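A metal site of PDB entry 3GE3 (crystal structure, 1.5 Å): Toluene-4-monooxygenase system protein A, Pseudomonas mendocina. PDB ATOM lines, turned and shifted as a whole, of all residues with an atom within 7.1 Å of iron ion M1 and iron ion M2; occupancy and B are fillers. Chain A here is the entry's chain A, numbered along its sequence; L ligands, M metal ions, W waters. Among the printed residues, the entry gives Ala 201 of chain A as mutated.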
ATOM      1  N   ILE A 100       8.490 -27.453  -9.131  1.00  0.00           N
ATOM      2  CA  ILE A 100       8.354 -26.022  -8.822  1.00  0.00           C
ATOM      3  C   ILE A 100       6.977 -25.582  -8.304  1.00  0.00           C
ATOM      4  O   ILE A 100       6.897 -24.781  -7.391  1.00  0.00           O
ATOM      5  CB  ILE A 100       8.733 -25.197 -10.109  1.00  0.00           C
ATOM      6  CG1 ILE A 100      10.210 -25.391 -10.425  1.00  0.00           C
ATOM      7  CG2 ILE A 100       8.344 -23.716  -9.968  1.00  0.00           C
ATOM      8  CD1 ILE A 100      11.150 -24.804  -9.395  1.00  0.00           C
ATOM      9  N   GLY A 103       6.180 -25.813  -4.599  1.00  0.00           N
ATOM     10  CA  GLY A 103       7.260 -25.072  -3.938  1.00  0.00           C
ATOM     11  C   GLY A 103       7.025 -23.557  -4.015  1.00  0.00           C
ATOM     12  O   GLY A 103       7.247 -22.845  -3.024  1.00  0.00           O
ATOM     13  N   GLU A 104       6.518 -23.066  -5.136  1.00  0.00           N
ATOM     14  CA  GLU A 104       6.128 -21.643  -5.224  1.00  0.00           C
ATOM     15  C   GLU A 104       5.068 -21.324  -4.180  1.00  0.00           C
ATOM     16  O   GLU A 104       5.125 -20.291  -3.483  1.00  0.00           O
ATOM     17  CB  GLU A 104       5.498 -21.397  -6.570  1.00  0.00           C
ATOM     18  CG  GLU A 104       6.404 -21.547  -7.746  1.00  0.00           C
ATOM     19  CD  GLU A 104       7.154 -20.296  -8.112  1.00  0.00           C
ATOM     20  OE1 GLU A 104       7.683 -20.286  -9.233  1.00  0.00           O
ATOM     21  OE2 GLU A 104       7.203 -19.339  -7.284  1.00  0.00           O
ATOM     22  N   TYR A 105       4.058 -22.190  -4.052  1.00  0.00           N
ATOM     23  CA  TYR A 105       3.044 -21.965  -3.053  1.00  0.00           C
ATOM     24  C   TYR A 105       3.656 -22.003  -1.629  1.00  0.00           C
ATOM     25  O   TYR A 105       3.268 -21.193  -0.780  1.00  0.00           O
ATOM     26  CB  TYR A 105       1.909 -22.999  -3.189  1.00  0.00           C
ATOM     27  CG  TYR A 105       0.799 -22.656  -2.264  1.00  0.00           C
ATOM     28  CD1 TYR A 105      -0.076 -21.561  -2.563  1.00  0.00           C
ATOM     29  CD2 TYR A 105       0.617 -23.328  -1.054  1.00  0.00           C
ATOM     30  CE1 TYR A 105      -1.098 -21.183  -1.675  1.00  0.00           C
ATOM     31  CE2 TYR A 105      -0.387 -22.976  -0.206  1.00  0.00           C
ATOM     32  CZ  TYR A 105      -1.242 -21.913  -0.470  1.00  0.00           C
ATOM     33  OH  TYR A 105      -2.207 -21.588   0.458  1.00  0.00           O
ATOM     34  N   ALA A 107       6.540 -20.913  -0.962  1.00  0.00           N
ATOM     35  CA  ALA A 107       7.251 -19.638  -0.853  1.00  0.00           C
ATOM     36  C   ALA A 107       6.337 -18.542  -0.305  1.00  0.00           C
ATOM     37  O   ALA A 107       6.834 -17.552   0.276  1.00  0.00           O
ATOM     38  CB  ALA A 107       7.859 -19.212  -2.170  1.00  0.00           C
ATOM     39  N   GLU A 111       7.450 -15.551   2.511  1.00  0.00           N
ATOM     40  CA  GLU A 111       7.090 -14.136   2.474  1.00  0.00           C
ATOM     41  C   GLU A 111       6.213 -13.765   3.650  1.00  0.00           C
ATOM     42  O   GLU A 111       6.406 -12.678   4.226  1.00  0.00           O
ATOM     43  CB  GLU A 111       6.411 -13.819   1.128  1.00  0.00           C
ATOM     44  CG  GLU A 111       7.298 -14.090  -0.134  1.00  0.00           C
ATOM     45  CD  GLU A 111       8.374 -13.014  -0.356  1.00  0.00           C
ATOM     46  OE1 GLU A 111       8.206 -11.886   0.078  1.00  0.00           O
ATOM     47  OE2 GLU A 111       9.429 -13.340  -0.930  1.00  0.00           O
ATOM     48  N   GLY A 130       5.038  -9.846  -1.876  1.00  0.00           N
ATOM     49  CA  GLY A 130       5.720 -11.136  -2.107  1.00  0.00           C
ATOM     50  C   GLY A 130       4.781 -12.311  -1.901  1.00  0.00           C
ATOM     51  O   GLY A 130       4.784 -13.272  -2.697  1.00  0.00           O
ATOM     52  N   ASP A 133       2.589 -12.486  -4.901  1.00  0.00           N
ATOM     53  CA  ASP A 133       3.342 -12.929  -6.084  1.00  0.00           C
ATOM     54  C   ASP A 133       3.510 -14.456  -6.030  1.00  0.00           C
ATOM     55  O   ASP A 133       3.366 -15.113  -7.069  1.00  0.00           O
ATOM     56  CB  ASP A 133       4.746 -12.350  -6.140  1.00  0.00           C
ATOM     57  CG  ASP A 133       4.791 -10.836  -6.379  1.00  0.00           C
ATOM     58  OD1 ASP A 133       3.850 -10.235  -6.936  1.00  0.00           O
ATOM     59  OD2 ASP A 133       5.848 -10.298  -6.078  1.00  0.00           O
ATOM     60  N   GLU A 134       3.875 -14.991  -4.858  1.00  0.00           N
ATOM     61  CA  GLU A 134       4.099 -16.424  -4.848  1.00  0.00           C
ATOM     62  C   GLU A 134       2.749 -17.179  -4.994  1.00  0.00           C
ATOM     63  O   GLU A 134       2.731 -18.308  -5.550  1.00  0.00           O
ATOM     64  CB  GLU A 134       4.840 -16.869  -3.597  1.00  0.00           C
ATOM     65  CG  GLU A 134       6.161 -16.180  -3.365  1.00  0.00           C
ATOM     66  CD  GLU A 134       7.220 -16.400  -4.419  1.00  0.00           C
ATOM     67  OE1 GLU A 134       6.955 -17.063  -5.433  1.00  0.00           O
ATOM     68  OE2 GLU A 134       8.388 -15.945  -4.173  1.00  0.00           O
ATOM     69  N   LEU A 135       1.644 -16.593  -4.516  1.00  0.00           N
ATOM     70  CA  LEU A 135       0.357 -17.184  -4.778  1.00  0.00           C
ATOM     71  C   LEU A 135       0.104 -17.251  -6.265  1.00  0.00           C
ATOM     72  O   LEU A 135      -0.309 -18.266  -6.780  1.00  0.00           O
ATOM     73  CB  LEU A 135      -0.734 -16.379  -4.084  1.00  0.00           C
ATOM     74  CG  LEU A 135      -2.162 -16.870  -4.284  1.00  0.00           C
ATOM     75  CD1 LEU A 135      -2.310 -18.281  -3.645  1.00  0.00           C
ATOM     76  CD2 LEU A 135      -3.169 -15.904  -3.719  1.00  0.00           C
ATOM     77  N   HIS A 137       2.343 -17.397  -8.602  1.00  0.00           N
ATOM     78  CA  HIS A 137       3.233 -18.369  -9.190  1.00  0.00           C
ATOM     79  C   HIS A 137       2.775 -19.813  -8.982  1.00  0.00           C
ATOM     80  O   HIS A 137       2.864 -20.627  -9.923  1.00  0.00           O
ATOM     81  CB  HIS A 137       4.648 -18.241  -8.625  1.00  0.00           C
ATOM     82  CG  HIS A 137       5.241 -16.892  -8.906  1.00  0.00           C
ATOM     83  ND1 HIS A 137       6.466 -16.491  -8.429  1.00  0.00           N
ATOM     84  CD2 HIS A 137       4.771 -15.894  -9.670  1.00  0.00           C
ATOM     85  CE1 HIS A 137       6.687 -15.239  -8.828  1.00  0.00           C
ATOM     86  NE2 HIS A 137       5.683 -14.865  -9.596  1.00  0.00           N
ATOM     87  N   GLY A 138       2.261 -20.076  -7.788  1.00  0.00           N
ATOM     88  CA  GLY A 138       1.785 -21.433  -7.501  1.00  0.00           C
ATOM     89  C   GLY A 138       0.527 -21.701  -8.330  1.00  0.00           C
ATOM     90  O   GLY A 138       0.358 -22.806  -8.901  1.00  0.00           O
ATOM     91  N   GLN A 141       1.314 -22.179 -12.124  1.00  0.00           N
ATOM     92  CA  GLN A 141       2.054 -23.405 -12.448  1.00  0.00           C
ATOM     93  C   GLN A 141       1.307 -24.691 -12.056  1.00  0.00           C
ATOM     94  O   GLN A 141       1.823 -25.774 -12.316  1.00  0.00           O
ATOM     95  CB  GLN A 141       3.448 -23.314 -11.839  1.00  0.00           C
ATOM     96  CG  GLN A 141       4.263 -22.283 -12.663  1.00  0.00           C
ATOM     97  CD  GLN A 141       5.578 -21.941 -12.044  1.00  0.00           C
ATOM     98  OE1 GLN A 141       5.642 -21.345 -10.934  1.00  0.00           O
ATOM     99  NE2 GLN A 141       6.602 -22.233 -12.751  1.00  0.00           N
ATOM    100  N   ILE A 180      13.432 -21.563   2.823  1.00  0.00           N
ATOM    101  CA  ILE A 180      12.219 -20.713   2.741  1.00  0.00           C
ATOM    102  C   ILE A 180      11.254 -20.862   3.875  1.00  0.00           C
ATOM    103  O   ILE A 180      10.827 -19.860   4.457  1.00  0.00           O
ATOM    104  CB  ILE A 180      11.451 -20.986   1.415  1.00  0.00           C
ATOM    105  CG1 ILE A 180      12.408 -20.796   0.261  1.00  0.00           C
ATOM    106  CG2 ILE A 180      10.196 -20.107   1.333  1.00  0.00           C
ATOM    107  CD1 ILE A 180      11.685 -20.989  -1.065  1.00  0.00           C
ATOM    108  N   LEU A 192      16.701 -16.697   0.755  1.00  0.00           N
ATOM    109  CA  LEU A 192      15.847 -16.957  -0.399  1.00  0.00           C
ATOM    110  C   LEU A 192      16.152 -15.966  -1.503  1.00  0.00           C
ATOM    111  O   LEU A 192      16.295 -16.342  -2.687  1.00  0.00           O
ATOM    112  CB  LEU A 192      14.398 -16.884   0.025  1.00  0.00           C
ATOM    113  CG  LEU A 192      13.357 -16.694  -1.086  1.00  0.00           C
ATOM    114  CD1 LEU A 192      13.390 -17.884  -2.030  1.00  0.00           C
ATOM    115  CD2 LEU A 192      11.978 -16.531  -0.496  1.00  0.00           C
ATOM    116  N   PHE A 196      18.005 -18.475  -4.608  1.00  0.00           N
ATOM    117  CA  PHE A 196      17.035 -18.773  -5.661  1.00  0.00           C
ATOM    118  C   PHE A 196      16.653 -17.494  -6.425  1.00  0.00           C
ATOM    119  O   PHE A 196      16.828 -17.413  -7.649  1.00  0.00           O
ATOM    120  CB  PHE A 196      15.799 -19.448  -5.077  1.00  0.00           C
ATOM    121  CG  PHE A 196      14.761 -19.749  -6.096  1.00  0.00           C
ATOM    122  CD1 PHE A 196      14.952 -20.733  -7.053  1.00  0.00           C
ATOM    123  CD2 PHE A 196      13.668 -18.958  -6.201  1.00  0.00           C
ATOM    124  CE1 PHE A 196      13.982 -20.957  -8.051  1.00  0.00           C
ATOM    125  CE2 PHE A 196      12.683 -19.184  -7.175  1.00  0.00           C
ATOM    126  CZ  PHE A 196      12.838 -20.172  -8.071  1.00  0.00           C
ATOM    127  N   GLU A 197      16.145 -16.460  -5.742  1.00  0.00           N
ATOM    128  CA  GLU A 197      15.382 -15.440  -6.484  1.00  0.00           C
ATOM    129  C   GLU A 197      16.217 -14.603  -7.433  1.00  0.00           C
ATOM    130  O   GLU A 197      15.803 -14.391  -8.559  1.00  0.00           O
ATOM    131  CB  GLU A 197      14.620 -14.532  -5.490  1.00  0.00           C
ATOM    132  CG  GLU A 197      13.642 -15.391  -4.687  1.00  0.00           C
ATOM    133  CD  GLU A 197      12.665 -14.571  -3.914  1.00  0.00           C
ATOM    134  OE1 GLU A 197      13.089 -13.531  -3.366  1.00  0.00           O
ATOM    135  OE2 GLU A 197      11.472 -14.953  -3.797  1.00  0.00           O
ATOM    136  N   ALA A 201      16.882 -18.989  -9.868  1.00  0.00           N
ATOM    137  CA  ALA A 201      15.622 -18.787 -10.573  1.00  0.00           C
ATOM    138  C   ALA A 201      15.878 -18.303 -11.976  1.00  0.00           C
ATOM    139  O   ALA A 201      15.134 -18.637 -12.902  1.00  0.00           O
ATOM    140  CB  ALA A 201      14.721 -17.776  -9.865  1.00  0.00           C
ATOM    141  N   PHE A 205      14.022 -20.153 -15.031  1.00  0.00           N
ATOM    142  CA  PHE A 205      12.902 -19.330 -15.541  1.00  0.00           C
ATOM    143  C   PHE A 205      13.250 -18.378 -16.722  1.00  0.00           C
ATOM    144  O   PHE A 205      12.316 -17.787 -17.382  1.00  0.00           O
ATOM    145  CB  PHE A 205      12.324 -18.493 -14.398  1.00  0.00           C
ATOM    146  CG  PHE A 205      11.552 -19.288 -13.390  1.00  0.00           C
ATOM    147  CD1 PHE A 205      12.245 -20.011 -12.438  1.00  0.00           C
ATOM    148  CD2 PHE A 205      10.175 -19.392 -13.449  1.00  0.00           C
ATOM    149  CE1 PHE A 205      11.530 -20.747 -11.482  1.00  0.00           C
ATOM    150  CE2 PHE A 205       9.464 -20.136 -12.517  1.00  0.00           C
ATOM    151  CZ  PHE A 205      10.149 -20.802 -11.549  1.00  0.00           C
ATOM    152  N   ILE A 227       6.687 -14.785 -14.754  1.00  0.00           N
ATOM    153  CA  ILE A 227       6.853 -15.088 -13.355  1.00  0.00           C
ATOM    154  C   ILE A 227       8.135 -14.374 -12.837  1.00  0.00           C
ATOM    155  O   ILE A 227       8.141 -13.789 -11.747  1.00  0.00           O
ATOM    156  CB  ILE A 227       6.887 -16.627 -13.177  1.00  0.00           C
ATOM    157  CG1 ILE A 227       5.450 -17.147 -13.336  1.00  0.00           C
ATOM    158  CG2 ILE A 227       7.561 -16.995 -11.846  1.00  0.00           C
ATOM    159  CD1 ILE A 227       5.382 -18.722 -13.289  1.00  0.00           C
ATOM    160  N   GLN A 228       9.219 -14.415 -13.623  1.00  0.00           N
ATOM    161  CA  GLN A 228      10.486 -13.835 -13.174  1.00  0.00           C
ATOM    162  C   GLN A 228      10.407 -12.314 -13.024  1.00  0.00           C
ATOM    163  O   GLN A 228      11.148 -11.770 -12.218  1.00  0.00           O
ATOM    164  CB  GLN A 228      11.637 -14.271 -14.079  1.00  0.00           C
ATOM    165  CG  GLN A 228      13.024 -14.145 -13.449  1.00  0.00           C
ATOM    166  CD  GLN A 228      13.247 -14.931 -12.164  1.00  0.00           C
ATOM    167  OE1 GLN A 228      12.434 -15.746 -11.755  1.00  0.00           O
ATOM    168  NE2 GLN A 228      14.371 -14.642 -11.508  1.00  0.00           N
ATOM    169  N   ASP A 230       8.077 -10.796 -11.450  1.00  0.00           N
ATOM    170  CA  ASP A 230       7.664 -10.539 -10.082  1.00  0.00           C
ATOM    171  C   ASP A 230       8.821 -10.802  -9.154  1.00  0.00           C
ATOM    172  O   ASP A 230       9.042 -10.049  -8.211  1.00  0.00           O
ATOM    173  CB  ASP A 230       6.576 -11.547  -9.689  1.00  0.00           C
ATOM    174  CG  ASP A 230       5.328 -11.461 -10.511  1.00  0.00           C
ATOM    175  OD1 ASP A 230       4.841 -10.367 -10.896  1.00  0.00           O
ATOM    176  OD2 ASP A 230       4.744 -12.525 -10.718  1.00  0.00           O
ATOM    177  N   GLU A 231       9.546 -11.914  -9.413  1.00  0.00           N
ATOM    178  CA  GLU A 231      10.724 -12.243  -8.634  1.00  0.00           C
ATOM    179  C   GLU A 231      11.709 -11.079  -8.565  1.00  0.00           C
ATOM    180  O   GLU A 231      12.299 -10.768  -7.520  1.00  0.00           O
ATOM    181  CB  GLU A 231      11.398 -13.470  -9.273  1.00  0.00           C
ATOM    182  CG  GLU A 231      12.485 -14.071  -8.453  1.00  0.00           C
ATOM    183  CD  GLU A 231      11.950 -15.204  -7.606  1.00  0.00           C
ATOM    184  OE1 GLU A 231      11.911 -16.350  -8.143  1.00  0.00           O
ATOM    185  OE2 GLU A 231      11.478 -14.980  -6.459  1.00  0.00           O
ATOM    186  N   SER A 232      11.937 -10.455  -9.718  1.00  0.00           N
ATOM    187  CA  SER A 232      12.952  -9.414  -9.814  1.00  0.00           C
ATOM    188  C   SER A 232      12.556  -8.218  -8.958  1.00  0.00           C
ATOM    189  O   SER A 232      13.420  -7.464  -8.511  1.00  0.00           O
ATOM    190  CB  SER A 232      13.208  -9.105 -11.278  1.00  0.00           C
ATOM    191  OG  SER A 232      13.942 -10.272 -11.726  1.00  0.00           O
ATOM    192  N   HIS A 234      10.253  -8.647  -5.937  1.00  0.00           N
ATOM    193  CA  HIS A 234      10.227  -8.982  -4.508  1.00  0.00           C
ATOM    194  C   HIS A 234      11.575  -9.456  -3.993  1.00  0.00           C
ATOM    195  O   HIS A 234      11.816  -9.394  -2.771  1.00  0.00           O
ATOM    196  CB  HIS A 234       9.073  -9.981  -4.146  1.00  0.00           C
ATOM    197  CG  HIS A 234       9.117 -11.359  -4.764  1.00  0.00           C
ATOM    198  ND1 HIS A 234       8.055 -11.841  -5.496  1.00  0.00           N
ATOM    199  CD2 HIS A 234      10.002 -12.387  -4.654  1.00  0.00           C
ATOM    200  CE1 HIS A 234       8.277 -13.099  -5.823  1.00  0.00           C
ATOM    201  NE2 HIS A 234       9.450 -13.475  -5.325  1.00  0.00           N
ATOM    202  N   ALA A 235      12.473  -9.885  -4.878  1.00  0.00           N
ATOM    203  CA  ALA A 235      13.824 -10.324  -4.417  1.00  0.00           C
ATOM    204  C   ALA A 235      14.596  -9.138  -3.879  1.00  0.00           C
ATOM    205  O   ALA A 235      15.604  -9.348  -3.170  1.00  0.00           O
ATOM    206  CB  ALA A 235      14.615 -10.953  -5.564  1.00  0.00           C
HETATM  207  C1  LIG L   1      10.286 -18.600  -5.103  1.00  0.00           C
HETATM  208  O1  LIG L   1      10.739 -17.449  -4.811  1.00  0.00           O
HETATM  209  O2  LIG L   1       9.357 -18.647  -5.955  1.00  0.00           O
HETATM  210  C2  LIG L   1      10.810 -19.813  -4.396  1.00  0.00           C
HETATM  211 FE    FE M   1      10.078 -15.555  -5.280  1.00  0.00          FE
HETATM  212 FE    FE M   2       8.041 -17.517  -7.167  1.00  0.00          FE
HETATM  213  O   HOH W   1       9.172 -18.131  -8.960  1.00  0.00           O
HETATM  214  O   HOH W   2       9.104 -15.874  -7.124  1.00  0.00           O
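Iron ion M1 is bound by OE2 of Glu 231 (1.9 Å), OE2 of Glu 134 (2.1 Å), O1 of the ligand (2.1 Å), water W2 (2.1 Å), OE2 of Glu 197 (2.1 Å) and NE2 of His 234 (2.2 Å).
Iron ion M2 is bound by water W2, the side-chain carboxylate (OE2) of Glu 104, the side-chain carboxylate (OE1) of Glu 134, an oxygen (O2) of the ligand, water W1 and a ring nitrogen (ND1) of His 137.
Three residues have an atom within 4 Å of iron ion M2: Glu 104, Glu 134 and His 137. Along chain A the residues within 4 Å of iron ion M2 span positions 104 to 137. The nearest printed residue that does not touch iron ion M2 is Glu 231 (4.2 Å).
Of the 26 residues printed, 4 come within 4 Å of iron ion M1. The nearest printed residue that does not touch iron ion M1 is Phe 196 (4.9 Å).
Water W1 lies within hydrogen-bond range of the side-chain carboxylate (OE1) of Glu 104 (2.6 Å) and the side-chain carboxylate (OE1) of Glu 231 (3.4 Å).
ND1 of His 234 sits at hydrogen-bond distance from OD2 of Asp 133 (2.8 Å). The side-chain amide nitrogen (NE2) of Gln 228 sits at hydrogen-bond distance from the backbone carbonyl oxygen (O) of Glu 197 (3.3 Å). The backbone carbonyl oxygen (O) of His 137 sits close to the side-chain amide oxygen (OE1) of Gln 141. The backbone carbonyl oxygen of Ile 227 sits at hydrogen-bond distance from a ring nitrogen (NE2) of His 137 (3.4 Å). A ring nitrogen (ND1) of His 234 is in hydrogen-bond range of the backbone carbonyl oxygen of Asp 230 (3.4 Å). NE2 of His 137 sits close to O of Asp 133 (3.4 Å). N of Glu 197 is in hydrogen-bond range of O of Leu 192 (3.1 Å). A ring nitrogen (NE2) of His 137 is in hydrogen-bond range of the side-chain carboxylate (OD2) of Asp 230 (2.8 Å).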
